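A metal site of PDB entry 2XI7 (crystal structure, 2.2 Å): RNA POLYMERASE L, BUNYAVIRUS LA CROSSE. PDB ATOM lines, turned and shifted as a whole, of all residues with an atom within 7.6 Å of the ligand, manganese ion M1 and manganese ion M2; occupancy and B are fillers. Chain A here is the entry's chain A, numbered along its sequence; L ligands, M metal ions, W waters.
The backbone carbonyl oxygen (O) of Ile 92 lies within hydrogen-bond range of the backbone NH (N) of Asp 80, 3.2 Å away.
OD2 of Asp 53 is in hydrogen-bond range of ND2 of Asn 52.
O of Pro 79 lies close to N of Asp 53 (3.4 Å).
The backbone NH of Ile 130 sits at hydrogen-bond distance from the backbone carbonyl oxygen of Asp 93 (2.9 Å).
The side-chain hydroxyl of Tyr 94 sits at hydrogen-bond distance from the side-chain amide nitrogen of Asn 81, 3.0 Å away.
OH of Tyr 94 lies within hydrogen-bond range of O of Arg 51, at 2.8 Å.
The side-chain carboxylate (OD1) of Asp 36 lies within hydrogen-bond range of a ring nitrogen (ND1) of His 35.
The side-chain amino group of Lys 95 sits at hydrogen-bond distance from the side-chain hydroxyl of Thr 106 (2.9 Å).
Manganese ion M1 is bound by O2 of the ligand (2.0 Å), OD2 of Asp 80 (2.0 Å), OD2 of Asp 93 (2.2 Å), O of Tyr 94 (2.2 Å), O1 of the ligand (2.2 Å) and NE2 of His 35 (2.3 Å).
Hydrophobic or aromatic side chains that line the ligand: His 35.
Of the 23 residues printed, 6 come within 4 Å of the ligand.
The nearest printed residue that does not touch the ligand is Thr 78 (4.9 Å).
NZ of Lys 95 is in salt-bridge range of O3 of the ligand (3.5 Å).
Two residues have an atom within 4 Å of manganese ion M2: Asp 53 and Asp 80.
The nearest printed residue that does not touch manganese ion M2 is Asp 93 (4.1 Å).
Manganese ion M2 is bound by OD1 of Asp 80, O1 of the ligand, O4 of the ligand, OD1 of Asp 53, water W2 and water W3.
Within 4 Å of manganese ion M1: His 35, Asp 80, Asp 93 and Tyr 94.
Water W3 lies within hydrogen-bond range of the side-chain amide oxygen of Asn 52 (2.7 Å) and the side-chain carboxylate of Asp 53 (3.1 Å).
Water W2 lies within hydrogen-bond range of the side-chain carboxylate of Asp 93 (2.7 Å), the backbone carbonyl oxygen of Thr 78 (2.8 Å), the backbone NH of Asp 80 (3.4 Å) and the side-chain hydroxyl of Tyr 110 (3.5 Å).
Water W1 lies within hydrogen-bond range of O3 of the ligand (2.5 Å) and NZ of Lys 95 (3.0 Å).
Water W4 bridges NZ of Lys 95 (3.4 Å) and OG1 of Thr 106 (3.4 Å).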
ATOM      1  N   LEU A  31      15.177   0.605  19.183  1.00  0.00           N
ATOM      2  CA  LEU A  31      14.773   0.785  20.573  1.00  0.00           C
ATOM      3  C   LEU A  31      13.618  -0.097  20.913  1.00  0.00           C
ATOM      4  O   LEU A  31      13.623  -0.691  21.994  1.00  0.00           O
ATOM      5  CB  LEU A  31      14.484   2.246  20.925  1.00  0.00           C
ATOM      6  CG  LEU A  31      15.723   3.155  20.890  1.00  0.00           C
ATOM      7  CD1 LEU A  31      15.395   4.658  21.100  1.00  0.00           C
ATOM      8  CD2 LEU A  31      16.744   2.702  21.947  1.00  0.00           C
ATOM      9  N   MET A  32      12.663  -0.261  20.017  1.00  0.00           N
ATOM     10  CA  MET A  32      11.526  -1.163  20.232  1.00  0.00           C
ATOM     11  C   MET A  32      12.006  -2.624  20.362  1.00  0.00           C
ATOM     12  O   MET A  32      11.597  -3.386  21.238  1.00  0.00           O
ATOM     13  CB  MET A  32      10.507  -1.019  19.066  1.00  0.00           C
ATOM     14  CG  MET A  32       9.742   0.329  19.038  1.00  0.00           C
ATOM     15  SD  MET A  32       8.442   0.567  17.762  1.00  0.00           S
ATOM     16  CE  MET A  32       8.245  -1.126  17.120  1.00  0.00           C
ATOM     17  N   HIS A  35      13.683  -3.270  23.663  1.00  0.00           N
ATOM     18  CA  HIS A  35      12.663  -3.374  24.699  1.00  0.00           C
ATOM     19  C   HIS A  35      12.048  -4.749  24.684  1.00  0.00           C
ATOM     20  O   HIS A  35      11.909  -5.384  25.733  1.00  0.00           O
ATOM     21  CB  HIS A  35      11.588  -2.282  24.482  1.00  0.00           C
ATOM     22  CG  HIS A  35      10.353  -2.434  25.310  1.00  0.00           C
ATOM     23  ND1 HIS A  35       9.338  -3.311  25.003  1.00  0.00           N
ATOM     24  CD2 HIS A  35       9.908  -1.719  26.387  1.00  0.00           C
ATOM     25  CE1 HIS A  35       8.342  -3.161  25.851  1.00  0.00           C
ATOM     26  NE2 HIS A  35       8.669  -2.193  26.696  1.00  0.00           N
ATOM     27  N   ASP A  36      11.633  -5.203  23.511  1.00  0.00           N
ATOM     28  CA  ASP A  36      10.985  -6.522  23.433  1.00  0.00           C
ATOM     29  C   ASP A  36      11.968  -7.693  23.777  1.00  0.00           C
ATOM     30  O   ASP A  36      11.601  -8.684  24.406  1.00  0.00           O
ATOM     31  CB  ASP A  36      10.347  -6.717  22.057  1.00  0.00           C
ATOM     32  CG  ASP A  36       9.230  -5.689  21.762  1.00  0.00           C
ATOM     33  OD1 ASP A  36       8.671  -5.050  22.704  1.00  0.00           O
ATOM     34  OD2 ASP A  36       8.898  -5.519  20.587  1.00  0.00           O
ATOM     35  N   ARG A  51       4.205 -11.692  27.385  1.00  0.00           N
ATOM     36  CA  ARG A  51       3.146 -10.932  26.722  1.00  0.00           C
ATOM     37  C   ARG A  51       3.675  -9.560  26.404  1.00  0.00           C
ATOM     38  O   ARG A  51       4.675  -9.131  26.987  1.00  0.00           O
ATOM     39  CB  ARG A  51       1.908 -10.784  27.599  1.00  0.00           C
ATOM     40  CG  ARG A  51       1.362 -12.061  28.242  1.00  0.00           C
ATOM     41  CD  ARG A  51       0.033 -11.755  28.931  1.00  0.00           C
ATOM     42  NE  ARG A  51      -0.634 -12.922  29.492  1.00  0.00           N
ATOM     43  CZ  ARG A  51      -0.411 -13.419  30.702  1.00  0.00           C
ATOM     44  NH1 ARG A  51       0.501 -12.865  31.521  1.00  0.00           N
ATOM     45  NH2 ARG A  51      -1.080 -14.479  31.103  1.00  0.00           N
ATOM     46  N   ASN A  52       3.015  -8.912  25.460  1.00  0.00           N
ATOM     47  CA  ASN A  52       3.275  -7.529  25.108  1.00  0.00           C
ATOM     48  C   ASN A  52       1.947  -6.790  24.942  1.00  0.00           C
ATOM     49  O   ASN A  52       1.030  -7.245  24.265  1.00  0.00           O
ATOM     50  CB  ASN A  52       4.068  -7.421  23.798  1.00  0.00           C
ATOM     51  CG  ASN A  52       4.694  -6.026  23.613  1.00  0.00           C
ATOM     52  OD1 ASN A  52       5.465  -5.558  24.454  1.00  0.00           O
ATOM     53  ND2 ASN A  52       4.338  -5.365  22.518  1.00  0.00           N
ATOM     54  N   ASP A  53       1.833  -5.645  25.568  1.00  0.00           N
ATOM     55  CA  ASP A  53       0.709  -4.786  25.367  1.00  0.00           C
ATOM     56  C   ASP A  53      -0.589  -5.572  25.441  1.00  0.00           C
ATOM     57  O   ASP A  53      -1.165  -5.939  24.402  1.00  0.00           O
ATOM     58  CB  ASP A  53       0.896  -4.056  24.035  1.00  0.00           C
ATOM     59  CG  ASP A  53       2.127  -3.154  24.077  1.00  0.00           C
ATOM     60  OD1 ASP A  53       2.719  -3.026  25.163  1.00  0.00           O
ATOM     61  OD2 ASP A  53       2.496  -2.566  23.039  1.00  0.00           O
ATOM     62  N   VAL A  54      -1.023  -5.865  26.660  1.00  0.00           N
ATOM     63  CA  VAL A  54      -2.269  -6.549  26.905  1.00  0.00           C
ATOM     64  C   VAL A  54      -3.309  -5.541  27.292  1.00  0.00           C
ATOM     65  O   VAL A  54      -3.106  -4.810  28.254  1.00  0.00           O
ATOM     66  CB  VAL A  54      -2.189  -7.546  28.093  1.00  0.00           C
ATOM     67  CG1 VAL A  54      -3.499  -8.391  28.145  1.00  0.00           C
ATOM     68  CG2 VAL A  54      -0.959  -8.419  27.947  1.00  0.00           C
ATOM     69  N   THR A  78      -2.728  -0.373  28.140  1.00  0.00           N
ATOM     70  CA  THR A  78      -2.208  -1.615  27.578  1.00  0.00           C
ATOM     71  C   THR A  78      -0.789  -1.847  28.073  1.00  0.00           C
ATOM     72  O   THR A  78       0.188  -1.684  27.347  1.00  0.00           O
ATOM     73  CB  THR A  78      -2.324  -1.601  26.034  1.00  0.00           C
ATOM     74  OG1 THR A  78      -1.348  -0.721  25.476  1.00  0.00           O
ATOM     75  CG2 THR A  78      -3.688  -1.087  25.645  1.00  0.00           C
ATOM     76  N   PRO A  79      -0.669  -2.273  29.347  1.00  0.00           N
ATOM     77  CA  PRO A  79       0.628  -2.605  29.929  1.00  0.00           C
ATOM     78  C   PRO A  79       1.300  -3.815  29.274  1.00  0.00           C
ATOM     79  O   PRO A  79       0.654  -4.636  28.609  1.00  0.00           O
ATOM     80  CB  PRO A  79       0.273  -2.912  31.391  1.00  0.00           C
ATOM     81  CG  PRO A  79      -1.076  -3.412  31.358  1.00  0.00           C
ATOM     82  CD  PRO A  79      -1.758  -2.548  30.289  1.00  0.00           C
ATOM     83  N   ASP A  80       2.602  -3.919  29.445  1.00  0.00           N
ATOM     84  CA  ASP A  80       3.337  -4.991  28.810  1.00  0.00           C
ATOM     85  C   ASP A  80       2.913  -6.366  29.278  1.00  0.00           C
ATOM     86  O   ASP A  80       2.866  -7.327  28.460  1.00  0.00           O
ATOM     87  CB  ASP A  80       4.868  -4.813  28.968  1.00  0.00           C
ATOM     88  CG  ASP A  80       5.407  -3.626  28.171  1.00  0.00           C
ATOM     89  OD1 ASP A  80       4.875  -3.389  27.091  1.00  0.00           O
ATOM     90  OD2 ASP A  80       6.345  -2.928  28.590  1.00  0.00           O
ATOM     91  N   ASN A  81       2.634  -6.511  30.570  1.00  0.00           N
ATOM     92  CA  ASN A  81       2.303  -7.816  31.115  1.00  0.00           C
ATOM     93  C   ASN A  81       1.620  -7.640  32.488  1.00  0.00           C
ATOM     94  O   ASN A  81       1.371  -6.514  32.922  1.00  0.00           O
ATOM     95  CB  ASN A  81       3.585  -8.645  31.253  1.00  0.00           C
ATOM     96  CG  ASN A  81       3.382 -10.154  31.057  1.00  0.00           C
ATOM     97  OD1 ASN A  81       2.292 -10.701  31.272  1.00  0.00           O
ATOM     98  ND2 ASN A  81       4.440 -10.835  30.643  1.00  0.00           N
ATOM     99  N   ILE A  92       2.654  -4.965  35.015  1.00  0.00           N
ATOM    100  CA  ILE A  92       4.084  -4.887  34.702  1.00  0.00           C
ATOM    101  C   ILE A  92       4.332  -4.130  33.403  1.00  0.00           C
ATOM    102  O   ILE A  92       3.644  -4.374  32.392  1.00  0.00           O
ATOM    103  CB  ILE A  92       4.681  -6.296  34.558  1.00  0.00           C
ATOM    104  CG1 ILE A  92       4.459  -7.079  35.849  1.00  0.00           C
ATOM    105  CG2 ILE A  92       6.152  -6.261  34.153  1.00  0.00           C
ATOM    106  CD1 ILE A  92       4.891  -8.562  35.761  1.00  0.00           C
ATOM    107  N   ASP A  93       5.305  -3.231  33.435  1.00  0.00           N
ATOM    108  CA  ASP A  93       5.794  -2.661  32.207  1.00  0.00           C
ATOM    109  C   ASP A  93       7.294  -2.767  32.158  1.00  0.00           C
ATOM    110  O   ASP A  93       7.983  -2.505  33.162  1.00  0.00           O
ATOM    111  CB  ASP A  93       5.344  -1.226  31.972  1.00  0.00           C
ATOM    112  CG  ASP A  93       5.180  -0.931  30.470  1.00  0.00           C
ATOM    113  OD1 ASP A  93       4.081  -1.242  29.872  1.00  0.00           O
ATOM    114  OD2 ASP A  93       6.186  -0.461  29.923  1.00  0.00           O
ATOM    115  N   TYR A  94       7.798  -3.167  30.995  1.00  0.00           N
ATOM    116  CA  TYR A  94       9.227  -3.300  30.777  1.00  0.00           C
ATOM    117  C   TYR A  94       9.758  -1.966  30.311  1.00  0.00           C
ATOM    118  O   TYR A  94       9.057  -1.301  29.540  1.00  0.00           O
ATOM    119  CB  TYR A  94       9.543  -4.313  29.656  1.00  0.00           C
ATOM    120  CG  TYR A  94       8.678  -5.555  29.567  1.00  0.00           C
ATOM    121  CD1 TYR A  94       8.419  -6.337  30.685  1.00  0.00           C
ATOM    122  CD2 TYR A  94       8.214  -6.002  28.338  1.00  0.00           C
ATOM    123  CE1 TYR A  94       7.652  -7.508  30.576  1.00  0.00           C
ATOM    124  CE2 TYR A  94       7.435  -7.168  28.209  1.00  0.00           C
ATOM    125  CZ  TYR A  94       7.140  -7.923  29.336  1.00  0.00           C
ATOM    126  OH  TYR A  94       6.368  -9.078  29.245  1.00  0.00           O
ATOM    127  N   LYS A  95      10.991  -1.626  30.703  1.00  0.00           N
ATOM    128  CA  LYS A  95      11.684  -0.461  30.244  1.00  0.00           C
ATOM    129  C   LYS A  95      13.158  -0.789  30.086  1.00  0.00           C
ATOM    130  O   LYS A  95      13.744  -1.550  30.920  1.00  0.00           O
ATOM    131  CB  LYS A  95      11.615   0.673  31.278  1.00  0.00           C
ATOM    132  CG  LYS A  95      10.219   1.178  31.516  1.00  0.00           C
ATOM    133  CD  LYS A  95       9.695   2.041  30.352  1.00  0.00           C
ATOM    134  CE  LYS A  95       8.210   2.392  30.611  1.00  0.00           C
ATOM    135  NZ  LYS A  95       7.617   3.113  29.514  1.00  0.00           N
ATOM    136  N   VAL A  96      13.770  -0.221  29.047  1.00  0.00           N
ATOM    137  CA  VAL A  96      15.213  -0.233  28.885  1.00  0.00           C
ATOM    138  C   VAL A  96      15.636   1.218  28.724  1.00  0.00           C
ATOM    139  O   VAL A  96      15.266   1.863  27.744  1.00  0.00           O
ATOM    140  CB  VAL A  96      15.681  -1.067  27.669  1.00  0.00           C
ATOM    141  CG1 VAL A  96      17.257  -1.055  27.548  1.00  0.00           C
ATOM    142  CG2 VAL A  96      15.102  -2.486  27.724  1.00  0.00           C
ATOM    143  N   SER A 102      11.055   7.843  31.575  1.00  0.00           N
ATOM    144  CA  SER A 102       9.986   7.133  30.920  1.00  0.00           C
ATOM    145  C   SER A 102       9.242   6.277  31.945  1.00  0.00           C
ATOM    146  O   SER A 102       8.049   6.079  31.811  1.00  0.00           O
ATOM    147  CB  SER A 102      10.533   6.297  29.752  1.00  0.00           C
ATOM    148  OG  SER A 102      11.337   5.219  30.243  1.00  0.00           O
ATOM    149  N   THR A 106       5.091   6.414  32.767  1.00  0.00           N
ATOM    150  CA  THR A 106       4.253   5.245  32.715  1.00  0.00           C
ATOM    151  C   THR A 106       3.705   4.962  34.102  1.00  0.00           C
ATOM    152  O   THR A 106       2.525   4.673  34.248  1.00  0.00           O
ATOM    153  CB  THR A 106       5.033   4.087  32.118  1.00  0.00           C
ATOM    154  OG1 THR A 106       5.410   4.475  30.786  1.00  0.00           O
ATOM    155  CG2 THR A 106       4.221   2.793  32.076  1.00  0.00           C
ATOM    156  N   LYS A 109       0.815   7.441  35.102  1.00  0.00           N
ATOM    157  CA  LYS A 109      -0.367   7.227  34.289  1.00  0.00           C
ATOM    158  C   LYS A 109      -1.099   5.960  34.786  1.00  0.00           C
ATOM    159  O   LYS A 109      -2.295   6.006  35.122  1.00  0.00           O
ATOM    160  CB  LYS A 109       0.065   7.108  32.833  1.00  0.00           C
ATOM    161  CG  LYS A 109      -1.067   7.132  31.821  1.00  0.00           C
ATOM    162  CD  LYS A 109      -0.738   6.223  30.634  1.00  0.00           C
ATOM    163  CE  LYS A 109       0.381   6.774  29.774  1.00  0.00           C
ATOM    164  NZ  LYS A 109       0.915   5.717  28.835  1.00  0.00           N
ATOM    165  N   TYR A 110      -0.372   4.849  34.888  1.00  0.00           N
ATOM    166  CA  TYR A 110      -1.002   3.577  35.261  1.00  0.00           C
ATOM    167  C   TYR A 110      -1.516   3.577  36.684  1.00  0.00           C
ATOM    168  O   TYR A 110      -2.587   3.026  36.961  1.00  0.00           O
ATOM    169  CB  TYR A 110      -0.041   2.396  35.102  1.00  0.00           C
ATOM    170  CG  TYR A 110       0.289   1.994  33.688  1.00  0.00           C
ATOM    171  CD1 TYR A 110      -0.264   2.646  32.583  1.00  0.00           C
ATOM    172  CD2 TYR A 110       1.140   0.915  33.457  1.00  0.00           C
ATOM    173  CE1 TYR A 110       0.032   2.247  31.270  1.00  0.00           C
ATOM    174  CE2 TYR A 110       1.458   0.510  32.164  1.00  0.00           C
ATOM    175  CZ  TYR A 110       0.889   1.186  31.065  1.00  0.00           C
ATOM    176  OH  TYR A 110       1.225   0.817  29.789  1.00  0.00           O
ATOM    177  N   ILE A 129       7.158  -1.219  37.464  1.00  0.00           N
ATOM    178  CA  ILE A 129       7.979  -0.839  36.353  1.00  0.00           C
ATOM    179  C   ILE A 129       9.325  -1.517  36.518  1.00  0.00           C
ATOM    180  O   ILE A 129      10.074  -1.227  37.492  1.00  0.00           O
ATOM    181  CB  ILE A 129       8.189   0.663  36.231  1.00  0.00           C
ATOM    182  CG1 ILE A 129       6.847   1.444  36.258  1.00  0.00           C
ATOM    183  CG2 ILE A 129       8.929   0.970  34.936  1.00  0.00           C
ATOM    184  CD1 ILE A 129       5.777   0.987  35.208  1.00  0.00           C
ATOM    185  N   ILE A 130       9.623  -2.454  35.601  1.00  0.00           N
ATOM    186  CA  ILE A 130      10.876  -3.185  35.610  1.00  0.00           C
ATOM    187  C   ILE A 130      11.791  -2.626  34.554  1.00  0.00           C
ATOM    188  O   ILE A 130      11.614  -2.866  33.354  1.00  0.00           O
ATOM    189  CB  ILE A 130      10.651  -4.696  35.398  1.00  0.00           C
ATOM    190  CG1 ILE A 130       9.629  -5.198  36.437  1.00  0.00           C
ATOM    191  CG2 ILE A 130      11.991  -5.434  35.572  1.00  0.00           C
ATOM    192  CD1 ILE A 130       9.211  -6.663  36.324  1.00  0.00           C
HETATM  193  O1  LIG L   1       5.871  -0.499  26.573  1.00  0.00           O
HETATM  194  C1  LIG L   1       6.414   0.608  26.055  1.00  0.00           C
HETATM  195  C2  LIG L   1       7.511   1.129  26.654  1.00  0.00           C
HETATM  196  O2  LIG L   1       8.002   0.573  27.679  1.00  0.00           O
HETATM  197  O3  LIG L   1       8.052   2.166  26.179  1.00  0.00           O
HETATM  198  C3  LIG L   1       5.874   1.238  24.985  1.00  0.00           C
HETATM  199  C4  LIG L   1       4.622   0.841  24.274  1.00  0.00           C
HETATM  200  C5  LIG L   1       4.035   1.809  23.261  1.00  0.00           C
HETATM  201  C6  LIG L   1       3.684   3.099  23.689  1.00  0.00           C
HETATM  202  C7  LIG L   1       3.112   4.032  22.800  1.00  0.00           C
HETATM  203  C8  LIG L   1       2.876   3.651  21.474  1.00  0.00           C
HETATM  204  C9  LIG L   1       3.227   2.361  21.046  1.00  0.00           C
HETATM  205  C10 LIG L   1       3.791   1.432  21.945  1.00  0.00           C
HETATM  206  O4  LIG L   1       3.949  -0.150  24.527  1.00  0.00           O
HETATM  207 MN    MN M   1       7.275  -1.198  28.179  1.00  0.00          MN
HETATM  208 MN    MN M   2       4.336  -1.781  25.854  1.00  0.00          MN
HETATM  209  O   HOH W   1       9.407   4.022  27.271  1.00  0.00           O
HETATM  210  O   HOH W   2       2.949  -1.133  27.473  1.00  0.00           O
HETATM  211  O   HOH W   3       5.387  -2.851  24.144  1.00  0.00           O
HETATM  212  O   HOH W   4       4.518   2.316  28.265  1.00  0.00           O
